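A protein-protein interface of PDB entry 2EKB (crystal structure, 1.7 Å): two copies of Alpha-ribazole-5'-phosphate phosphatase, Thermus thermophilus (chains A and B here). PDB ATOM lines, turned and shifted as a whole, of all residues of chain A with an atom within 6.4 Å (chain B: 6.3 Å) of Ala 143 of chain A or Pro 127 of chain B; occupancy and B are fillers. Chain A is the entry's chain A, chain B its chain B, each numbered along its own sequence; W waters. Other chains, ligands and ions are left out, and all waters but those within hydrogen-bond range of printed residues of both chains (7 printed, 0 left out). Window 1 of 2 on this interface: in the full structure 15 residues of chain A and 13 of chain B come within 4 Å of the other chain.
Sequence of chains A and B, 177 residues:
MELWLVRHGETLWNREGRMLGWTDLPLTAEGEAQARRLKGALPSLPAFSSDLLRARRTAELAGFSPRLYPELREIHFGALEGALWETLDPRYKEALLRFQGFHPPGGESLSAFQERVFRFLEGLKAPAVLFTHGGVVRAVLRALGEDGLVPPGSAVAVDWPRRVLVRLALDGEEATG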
ATOM      1  N   PHE A 118     -23.201 -16.570  22.914  1.00  0.00           N
ATOM      2  CA  PHE A 118     -21.829 -16.651  22.437  1.00  0.00           C
ATOM      3  C   PHE A 118     -21.664 -17.544  21.216  1.00  0.00           C
ATOM      4  O   PHE A 118     -20.793 -17.300  20.387  1.00  0.00           O
ATOM      5  CB  PHE A 118     -20.902 -17.094  23.571  1.00  0.00           C
ATOM      6  CG  PHE A 118     -20.922 -16.164  24.754  1.00  0.00           C
ATOM      7  CD1 PHE A 118     -21.114 -14.793  24.570  1.00  0.00           C
ATOM      8  CD2 PHE A 118     -20.750 -16.650  26.045  1.00  0.00           C
ATOM      9  CE1 PHE A 118     -21.135 -13.916  25.660  1.00  0.00           C
ATOM     10  CE2 PHE A 118     -20.769 -15.778  27.146  1.00  0.00           C
ATOM     11  CZ  PHE A 118     -20.961 -14.413  26.948  1.00  0.00           C
ATOM     12  N   ARG A 138     -25.429  -7.176  28.285  1.00  0.00           N
ATOM     13  CA  ARG A 138     -24.784  -7.362  29.578  1.00  0.00           C
ATOM     14  C   ARG A 138     -23.852  -8.570  29.564  1.00  0.00           C
ATOM     15  O   ARG A 138     -22.726  -8.498  30.054  1.00  0.00           O
ATOM     16  CB  ARG A 138     -25.833  -7.528  30.681  1.00  0.00           C
ATOM     17  CG  ARG A 138     -25.239  -7.543  32.071  1.00  0.00           C
ATOM     18  CD  ARG A 138     -26.300  -7.758  33.131  1.00  0.00           C
ATOM     19  NE  ARG A 138     -25.695  -7.784  34.458  1.00  0.00           N
ATOM     20  CZ  ARG A 138     -26.303  -8.233  35.551  1.00  0.00           C
ATOM     21  NH1 ARG A 138     -27.544  -8.700  35.483  1.00  0.00           N
ATOM     22  NH2 ARG A 138     -25.658  -8.222  36.709  1.00  0.00           N
ATOM     23  N   ALA A 139     -24.316  -9.682  28.999  1.00  0.00           N
ATOM     24  CA  ALA A 139     -23.499 -10.889  28.943  1.00  0.00           C
ATOM     25  C   ALA A 139     -22.192 -10.609  28.203  1.00  0.00           C
ATOM     26  O   ALA A 139     -21.120 -11.026  28.638  1.00  0.00           O
ATOM     27  CB  ALA A 139     -24.271 -12.020  28.251  1.00  0.00           C
ATOM     28  N   VAL A 140     -22.294  -9.887  27.092  1.00  0.00           N
ATOM     29  CA  VAL A 140     -21.124  -9.557  26.290  1.00  0.00           C
ATOM     30  C   VAL A 140     -20.181  -8.607  27.030  1.00  0.00           C
ATOM     31  O   VAL A 140     -18.977  -8.855  27.104  1.00  0.00           O
ATOM     32  CB  VAL A 140     -21.548  -8.924  24.941  1.00  0.00           C
ATOM     33  CG1 VAL A 140     -20.331  -8.382  24.190  1.00  0.00           C
ATOM     34  CG2 VAL A 140     -22.255  -9.975  24.090  1.00  0.00           C
ATOM     35  N   LEU A 141     -20.724  -7.532  27.591  1.00  0.00           N
ATOM     36  CA  LEU A 141     -19.878  -6.578  28.303  1.00  0.00           C
ATOM     37  C   LEU A 141     -19.192  -7.225  29.504  1.00  0.00           C
ATOM     38  O   LEU A 141     -17.997  -7.023  29.722  1.00  0.00           O
ATOM     39  CB  LEU A 141     -20.695  -5.363  28.749  1.00  0.00           C
ATOM     40  CG  LEU A 141     -21.213  -4.474  27.611  1.00  0.00           C
ATOM     41  CD1 LEU A 141     -21.952  -3.279  28.191  1.00  0.00           C
ATOM     42  CD2 LEU A 141     -20.049  -4.013  26.736  1.00  0.00           C
ATOM     43  N   ARG A 142     -19.940  -8.013  30.271  1.00  0.00           N
ATOM     44  CA  ARG A 142     -19.375  -8.678  31.440  1.00  0.00           C
ATOM     45  C   ARG A 142     -18.276  -9.664  31.050  1.00  0.00           C
ATOM     46  O   ARG A 142     -17.263  -9.794  31.751  1.00  0.00           O
ATOM     47  CB  ARG A 142     -20.466  -9.418  32.224  1.00  0.00           C
ATOM     48  CG  ARG A 142     -21.439  -8.519  32.962  1.00  0.00           C
ATOM     49  CD  ARG A 142     -22.368  -9.351  33.839  1.00  0.00           C
ATOM     50  NE  ARG A 142     -21.652 -10.055  34.903  1.00  0.00           N
ATOM     51  CZ  ARG A 142     -21.440  -9.558  36.122  1.00  0.00           C
ATOM     52  NH1 ARG A 142     -21.887  -8.352  36.441  1.00  0.00           N
ATOM     53  NH2 ARG A 142     -20.783 -10.272  37.024  1.00  0.00           N
ATOM     54  N   ALA A 143     -18.469 -10.358  29.931  1.00  0.00           N
ATOM     55  CA  ALA A 143     -17.461 -11.314  29.496  1.00  0.00           C
ATOM     56  C   ALA A 143     -16.172 -10.595  29.106  1.00  0.00           C
ATOM     57  O   ALA A 143     -15.079 -11.136  29.149  1.00  0.00           O
ATOM     58  CB  ALA A 143     -18.025 -12.077  28.297  1.00  0.00           C
ATOM     59  N   LEU A 144     -16.350  -9.333  28.680  1.00  0.00           N
ATOM     60  CA  LEU A 144     -15.197  -8.512  28.334  1.00  0.00           C
ATOM     61  C   LEU A 144     -14.678  -7.731  29.545  1.00  0.00           C
ATOM     62  O   LEU A 144     -13.908  -6.789  29.430  1.00  0.00           O
ATOM     63  CB  LEU A 144     -15.616  -7.546  27.228  1.00  0.00           C
ATOM     64  CG  LEU A 144     -15.942  -8.265  25.911  1.00  0.00           C
ATOM     65  CD1 LEU A 144     -16.323  -7.291  24.791  1.00  0.00           C
ATOM     66  CD2 LEU A 144     -14.770  -9.083  25.373  1.00  0.00           C
ATOM     67  N   GLY A 145     -15.179  -8.123  30.740  1.00  0.00           N
ATOM     68  CA  GLY A 145     -14.626  -7.597  31.991  1.00  0.00           C
ATOM     69  C   GLY A 145     -15.129  -6.192  32.341  1.00  0.00           C
ATOM     70  O   GLY A 145     -14.500  -5.448  33.083  1.00  0.00           O
ATOM     71  N   GLU A 146     -16.283  -5.759  31.846  1.00  0.00           N
ATOM     72  CA  GLU A 146     -16.791  -4.430  32.185  1.00  0.00           C
ATOM     73  C   GLU A 146     -18.224  -4.496  32.705  1.00  0.00           C
ATOM     74  O   GLU A 146     -18.903  -5.510  32.541  1.00  0.00           O
ATOM     75  CB  GLU A 146     -16.750  -3.508  30.960  1.00  0.00           C
ATOM     76  CG  GLU A 146     -15.409  -3.498  30.233  1.00  0.00           C
ATOM     77  CD  GLU A 146     -15.231  -2.299  29.317  1.00  0.00           C
ATOM     78  OE1 GLU A 146     -16.235  -1.653  28.957  1.00  0.00           O
ATOM     79  OE2 GLU A 146     -14.075  -2.011  28.947  1.00  0.00           O
ATOM     80  N   TRP A 160     -15.000  -8.310  19.341  1.00  0.00           N
ATOM     81  CA  TRP A 160     -15.257  -9.610  19.938  1.00  0.00           C
ATOM     82  C   TRP A 160     -14.233 -10.652  19.529  1.00  0.00           C
ATOM     83  O   TRP A 160     -13.907 -10.768  18.347  1.00  0.00           O
ATOM     84  CB  TRP A 160     -16.664 -10.067  19.544  1.00  0.00           C
ATOM     85  CG  TRP A 160     -17.069 -11.326  20.200  1.00  0.00           C
ATOM     86  CD1 TRP A 160     -17.151 -12.559  19.626  1.00  0.00           C
ATOM     87  CD2 TRP A 160     -17.401 -11.499  21.580  1.00  0.00           C
ATOM     88  NE1 TRP A 160     -17.512 -13.495  20.565  1.00  0.00           N
ATOM     89  CE2 TRP A 160     -17.672 -12.871  21.774  1.00  0.00           C
ATOM     90  CE3 TRP A 160     -17.494 -10.628  22.676  1.00  0.00           C
ATOM     91  CZ2 TRP A 160     -18.027 -13.394  23.017  1.00  0.00           C
ATOM     92  CZ3 TRP A 160     -17.848 -11.151  23.916  1.00  0.00           C
ATOM     93  CH2 TRP A 160     -18.109 -12.524  24.076  1.00  0.00           C
ATOM     94  N   PRO A 161     -13.724 -11.445  20.493  1.00  0.00           N
ATOM     95  CA  PRO A 161     -13.987 -11.497  21.938  1.00  0.00           C
ATOM     96  C   PRO A 161     -12.825 -10.919  22.753  1.00  0.00           C
ATOM     97  O   PRO A 161     -12.371 -11.531  23.729  1.00  0.00           O
ATOM     98  CB  PRO A 161     -14.127 -12.986  22.175  1.00  0.00           C
ATOM     99  CG  PRO A 161     -12.961 -13.506  21.364  1.00  0.00           C
ATOM    100  CD  PRO A 161     -13.014 -12.668  20.069  1.00  0.00           C
ATOM    101  N   ARG A 162     -12.360  -9.737  22.365  1.00  0.00           N
ATOM    102  CA  ARG A 162     -11.218  -9.124  23.028  1.00  0.00           C
ATOM    103  C   ARG A 162     -11.473  -7.885  23.887  1.00  0.00           C
ATOM    104  O   ARG A 162     -11.008  -7.825  25.025  1.00  0.00           O
ATOM    105  CB  ARG A 162     -10.147  -8.805  21.975  1.00  0.00           C
ATOM    106  CG  ARG A 162      -9.701 -10.021  21.155  1.00  0.00           C
ATOM    107  CD  ARG A 162      -8.599  -9.665  20.154  1.00  0.00           C
ATOM    108  NE  ARG A 162      -7.391  -9.187  20.824  1.00  0.00           N
ATOM    109  CZ  ARG A 162      -6.527  -9.967  21.471  1.00  0.00           C
ATOM    110  NH1 ARG A 162      -6.720 -11.275  21.539  1.00  0.00           N
ATOM    111  NH2 ARG A 162      -5.476  -9.431  22.079  1.00  0.00           N
ATOM    112  N   MET B   1      -8.058 -14.263  23.364  1.00  0.00           N
ATOM    113  CA  MET B   1      -9.232 -14.268  24.287  1.00  0.00           C
ATOM    114  C   MET B   1      -8.762 -14.537  25.715  1.00  0.00           C
ATOM    115  O   MET B   1      -8.034 -15.499  25.969  1.00  0.00           O
ATOM    116  CB  MET B   1     -10.227 -15.335  23.843  1.00  0.00           C
ATOM    117  CG  MET B   1     -11.591 -15.207  24.485  1.00  0.00           C
ATOM    118  SD  MET B   1     -12.777 -16.269  23.664  1.00  0.00           S
ATOM    119  CE  MET B   1     -12.289 -17.866  24.298  1.00  0.00           C
ATOM    120  N   GLU B   2      -9.188 -13.683  26.638  1.00  0.00           N
ATOM    121  CA  GLU B   2      -8.784 -13.777  28.035  1.00  0.00           C
ATOM    122  C   GLU B   2      -9.334 -14.983  28.791  1.00  0.00           C
ATOM    123  O   GLU B   2     -10.546 -15.162  28.902  1.00  0.00           O
ATOM    124  CB  GLU B   2      -9.182 -12.492  28.770  1.00  0.00           C
ATOM    125  CG  GLU B   2      -8.589 -12.369  30.168  1.00  0.00           C
ATOM    126  CD  GLU B   2      -8.819 -10.999  30.784  1.00  0.00           C
ATOM    127  OE1 GLU B   2      -8.764 -10.000  30.036  1.00  0.00           O
ATOM    128  OE2 GLU B   2      -9.043 -10.916  32.009  1.00  0.00           O
ATOM    129  N   LEU B   3      -8.421 -15.803  29.308  1.00  0.00           N
ATOM    130  CA  LEU B   3      -8.782 -16.979  30.087  1.00  0.00           C
ATOM    131  C   LEU B   3      -7.990 -16.959  31.379  1.00  0.00           C
ATOM    132  O   LEU B   3      -6.788 -16.701  31.378  1.00  0.00           O
ATOM    133  CB  LEU B   3      -8.441 -18.272  29.342  1.00  0.00           C
ATOM    134  CG  LEU B   3      -9.045 -18.502  27.964  1.00  0.00           C
ATOM    135  CD1 LEU B   3      -8.576 -19.860  27.463  1.00  0.00           C
ATOM    136  CD2 LEU B   3     -10.563 -18.443  28.026  1.00  0.00           C
ATOM    137  N   SER B  44     -15.243 -11.293  37.129  1.00  0.00           N
ATOM    138  CA  SER B  44     -16.533 -11.972  37.029  1.00  0.00           C
ATOM    139  C   SER B  44     -16.911 -12.386  35.612  1.00  0.00           C
ATOM    140  O   SER B  44     -17.895 -11.903  35.052  1.00  0.00           O
ATOM    141  CB  SER B  44     -17.630 -11.080  37.623  1.00  0.00           C
ATOM    142  OG  SER B  44     -17.529  -9.761  37.112  1.00  0.00           O
ATOM    143  N   LEU B  45     -16.126 -13.291  35.041  1.00  0.00           N
ATOM    144  CA  LEU B  45     -16.370 -13.789  33.693  1.00  0.00           C
ATOM    145  C   LEU B  45     -17.095 -15.124  33.806  1.00  0.00           C
ATOM    146  O   LEU B  45     -17.228 -15.670  34.906  1.00  0.00           O
ATOM    147  CB  LEU B  45     -15.037 -14.013  32.969  1.00  0.00           C
ATOM    148  CG  LEU B  45     -13.983 -12.906  33.083  1.00  0.00           C
ATOM    149  CD1 LEU B  45     -12.737 -13.302  32.309  1.00  0.00           C
ATOM    150  CD2 LEU B  45     -14.548 -11.597  32.556  1.00  0.00           C
ATOM    151  N   PRO B  46     -17.590 -15.659  32.675  1.00  0.00           N
ATOM    152  CA  PRO B  46     -18.284 -16.950  32.708  1.00  0.00           C
ATOM    153  C   PRO B  46     -17.312 -17.948  33.338  1.00  0.00           C
ATOM    154  O   PRO B  46     -16.116 -17.934  33.023  1.00  0.00           O
ATOM    155  CB  PRO B  46     -18.528 -17.247  31.231  1.00  0.00           C
ATOM    156  CG  PRO B  46     -18.752 -15.878  30.656  1.00  0.00           C
ATOM    157  CD  PRO B  46     -17.669 -15.049  31.332  1.00  0.00           C
ATOM    158  N   ALA B  47     -17.812 -18.807  34.222  1.00  0.00           N
ATOM    159  CA  ALA B  47     -16.943 -19.761  34.893  1.00  0.00           C
ATOM    160  C   ALA B  47     -17.171 -21.215  34.505  1.00  0.00           C
ATOM    161  O   ALA B  47     -18.294 -21.633  34.213  1.00  0.00           O
ATOM    162  CB  ALA B  47     -17.088 -19.599  36.399  1.00  0.00           C
ATOM    163  N   PHE B  48     -16.081 -21.975  34.508  1.00  0.00           N
ATOM    164  CA  PHE B  48     -16.096 -23.397  34.188  1.00  0.00           C
ATOM    165  C   PHE B  48     -15.198 -24.049  35.219  1.00  0.00           C
ATOM    166  O   PHE B  48     -14.300 -23.405  35.771  1.00  0.00           O
ATOM    167  CB  PHE B  48     -15.526 -23.654  32.790  1.00  0.00           C
ATOM    168  CG  PHE B  48     -16.334 -23.049  31.682  1.00  0.00           C
ATOM    169  CD1 PHE B  48     -16.151 -21.718  31.321  1.00  0.00           C
ATOM    170  CD2 PHE B  48     -17.298 -23.799  31.013  1.00  0.00           C
ATOM    171  CE1 PHE B  48     -16.915 -21.139  30.309  1.00  0.00           C
ATOM    172  CE2 PHE B  48     -18.068 -23.232  29.998  1.00  0.00           C
ATOM    173  CZ  PHE B  48     -17.877 -21.896  29.645  1.00  0.00           C
ATOM    174  N   LYS B 125     -16.066 -20.116  23.675  1.00  0.00           N
ATOM    175  CA  LYS B 125     -16.594 -19.090  22.784  1.00  0.00           C
ATOM    176  C   LYS B 125     -16.586 -17.684  23.371  1.00  0.00           C
ATOM    177  O   LYS B 125     -17.100 -16.745  22.762  1.00  0.00           O
ATOM    178  CB  LYS B 125     -18.022 -19.466  22.385  1.00  0.00           C
ATOM    179  CG  LYS B 125     -18.121 -20.833  21.720  1.00  0.00           C
ATOM    180  CD  LYS B 125     -19.561 -21.235  21.468  1.00  0.00           C
ATOM    181  CE  LYS B 125     -19.617 -22.509  20.636  1.00  0.00           C
ATOM    182  NZ  LYS B 125     -18.851 -23.621  21.267  1.00  0.00           N
ATOM    183  N   ALA B 126     -16.010 -17.542  24.558  1.00  0.00           N
ATOM    184  CA  ALA B 126     -15.939 -16.244  25.203  1.00  0.00           C
ATOM    185  C   ALA B 126     -14.937 -16.308  26.347  1.00  0.00           C
ATOM    186  O   ALA B 126     -14.539 -17.397  26.766  1.00  0.00           O
ATOM    187  CB  ALA B 126     -17.323 -15.851  25.727  1.00  0.00           C
ATOM    188  N   PRO B 127     -14.487 -15.143  26.844  1.00  0.00           N
ATOM    189  CA  PRO B 127     -13.531 -15.118  27.958  1.00  0.00           C
ATOM    190  C   PRO B 127     -14.101 -15.921  29.123  1.00  0.00           C
ATOM    191  O   PRO B 127     -15.324 -16.020  29.283  1.00  0.00           O
ATOM    192  CB  PRO B 127     -13.424 -13.633  28.279  1.00  0.00           C
ATOM    193  CG  PRO B 127     -13.556 -13.006  26.916  1.00  0.00           C
ATOM    194  CD  PRO B 127     -14.731 -13.781  26.337  1.00  0.00           C
ATOM    195  N   ALA B 128     -13.230 -16.471  29.960  1.00  0.00           N
ATOM    196  CA  ALA B 128     -13.721 -17.283  31.063  1.00  0.00           C
ATOM    197  C   ALA B 128     -12.718 -17.478  32.183  1.00  0.00           C
ATOM    198  O   ALA B 128     -11.520 -17.230  32.021  1.00  0.00           O
ATOM    199  CB  ALA B 128     -14.138 -18.655  30.525  1.00  0.00           C
ATOM    200  N   VAL B 129     -13.236 -17.925  33.324  1.00  0.00           N
ATOM    201  CA  VAL B 129     -12.405 -18.251  34.476  1.00  0.00           C
ATOM    202  C   VAL B 129     -12.538 -19.766  34.564  1.00  0.00           C
ATOM    203  O   VAL B 129     -13.661 -20.301  34.613  1.00  0.00           O
ATOM    204  CB  VAL B 129     -12.918 -17.593  35.775  1.00  0.00           C
ATOM    205  CG1 VAL B 129     -12.114 -18.110  36.970  1.00  0.00           C
ATOM    206  CG2 VAL B 129     -12.775 -16.070  35.674  1.00  0.00           C
HETATM  207  O   HOH W   1     -10.985  -9.546  27.912  1.00  0.00           O
HETATM  208  O   HOH W   2     -20.746 -13.052  36.587  1.00  0.00           O
HETATM  209  O   HOH W   3     -17.123  -8.949  34.396  1.00  0.00           O
HETATM  210  O   HOH W   4      -8.895 -13.410  20.606  1.00  0.00           O
HETATM  211  O   HOH W   5     -20.154 -12.822  33.452  1.00  0.00           O
HETATM  212  O   HOH W   6     -10.566 -11.356  25.894  1.00  0.00           O
HETATM  213  O   HOH W   7     -18.228 -16.340  20.462  1.00  0.00           O
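The side-chain hydroxyl (OG) of Ser 44 of chain B lies within hydrogen-bond range of the guanidinium group (NH2) of Arg 142 of chain A (3.3 Å).
Arg 138 of chain A touches none of the printed residues of chain B. Printed residues of chain B within 4 Å of Arg 142 of chain A: Ser 44 (3.3 Å) and Leu 45 (3.4 Å). Ala 143 of chain A touches two residues of chain B. Of the printed residues of chain B, Pro 161 of chain A touches Met 1 (3.6 Å) and Pro 127 (3.7 Å). Of the printed residues of chain A, Leu 45 of chain B touches Arg 142, Ala 143 and Gly 145. Printed residues of chain A within 4 Å of Ala 126 of chain B: Phe 118 (3.5 Å) and Trp 160 (3.7 Å). Of chain A, only Ala 143 (3.1 Å) and Pro 161 (3.7 Å) come within 4 Å of Pro 127 of chain B. The nearest residue of chain A that does not touch Pro 127 of chain B is Trp 160 of chain A (4.3 Å). The nearest printed residue of chain A that does not touch Met 1 of chain B is Trp 160 of chain A (6.0 Å).
Water W7 lies within hydrogen-bond range of the backbone carbonyl oxygen of Lys 125 of chain B (2.6 Å), the backbone carbonyl oxygen of Phe 118 of chain A (2.7 Å) and the indole nitrogen of Trp 160 of chain A (2.9 Å). Water W3 lies within hydrogen-bond range of O of Arg 142 of chain A (2.8 Å) and OG of Ser 44 of chain B (2.9 Å). Water W6 bridges N of Glu 2 of chain B and O of Pro 161 of chain A. Water W2 bridges the guanidinium group of Arg 142 of chain A (2.8 Å) and the backbone carbonyl oxygen of Ser 44 of chain B (3.4 Å). Water W5 bridges O of Ser 44 of chain B (2.9 Å) and NE of Arg 142 of chain A (3.5 Å). Water W1 lies within hydrogen-bond range of the side-chain carboxylate of Glu 2 of chain B (3.1 Å) and the backbone carbonyl oxygen of Arg 162 of chain A (3.4 Å).
The side-chain sulfur (SD) of Met 1 of chain B lies close to the backbone NH (N) of Ala 126 of chain B (3.6 Å).
Lys 125 of chain B touches Phe 118 of chain A. CD2 of Phe 118 of chain A touches CB of Ala 126 of chain B (3.5 Å). Leu 45 of chain B touches Arg 142 of chain A. Leu 45 of chain B touches Ala 143 of chain A. Pro 127 of chain B touches Ala 143 of chain A (CB to O, 3.1 Å). N of Gly 145 of chain A touches CD2 of Leu 45 of chain B (3.97 Å). O of Lys 125 of chain B touches CZ2 of Trp 160 of chain A, 3.5 Å away. CG of Pro 161 of chain A touches SD of Met 1 of chain B, at 3.6 Å. Pro 127 of chain B touches Pro 161 of chain A. Met 1 of chain B touches Arg 162 of chain A (N to NH1, 3.7 Å).
No position is printed for both chains.
Along chain B the printed residues that touch a printed residue of chain A span positions 1 to 127. Hydrophobic or aromatic side chains of chain A within 4 Å of the printed part of chain B: Phe 118, Trp 160 and Pro 161. Among the printed residues, 12 pairs touch across the chains.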
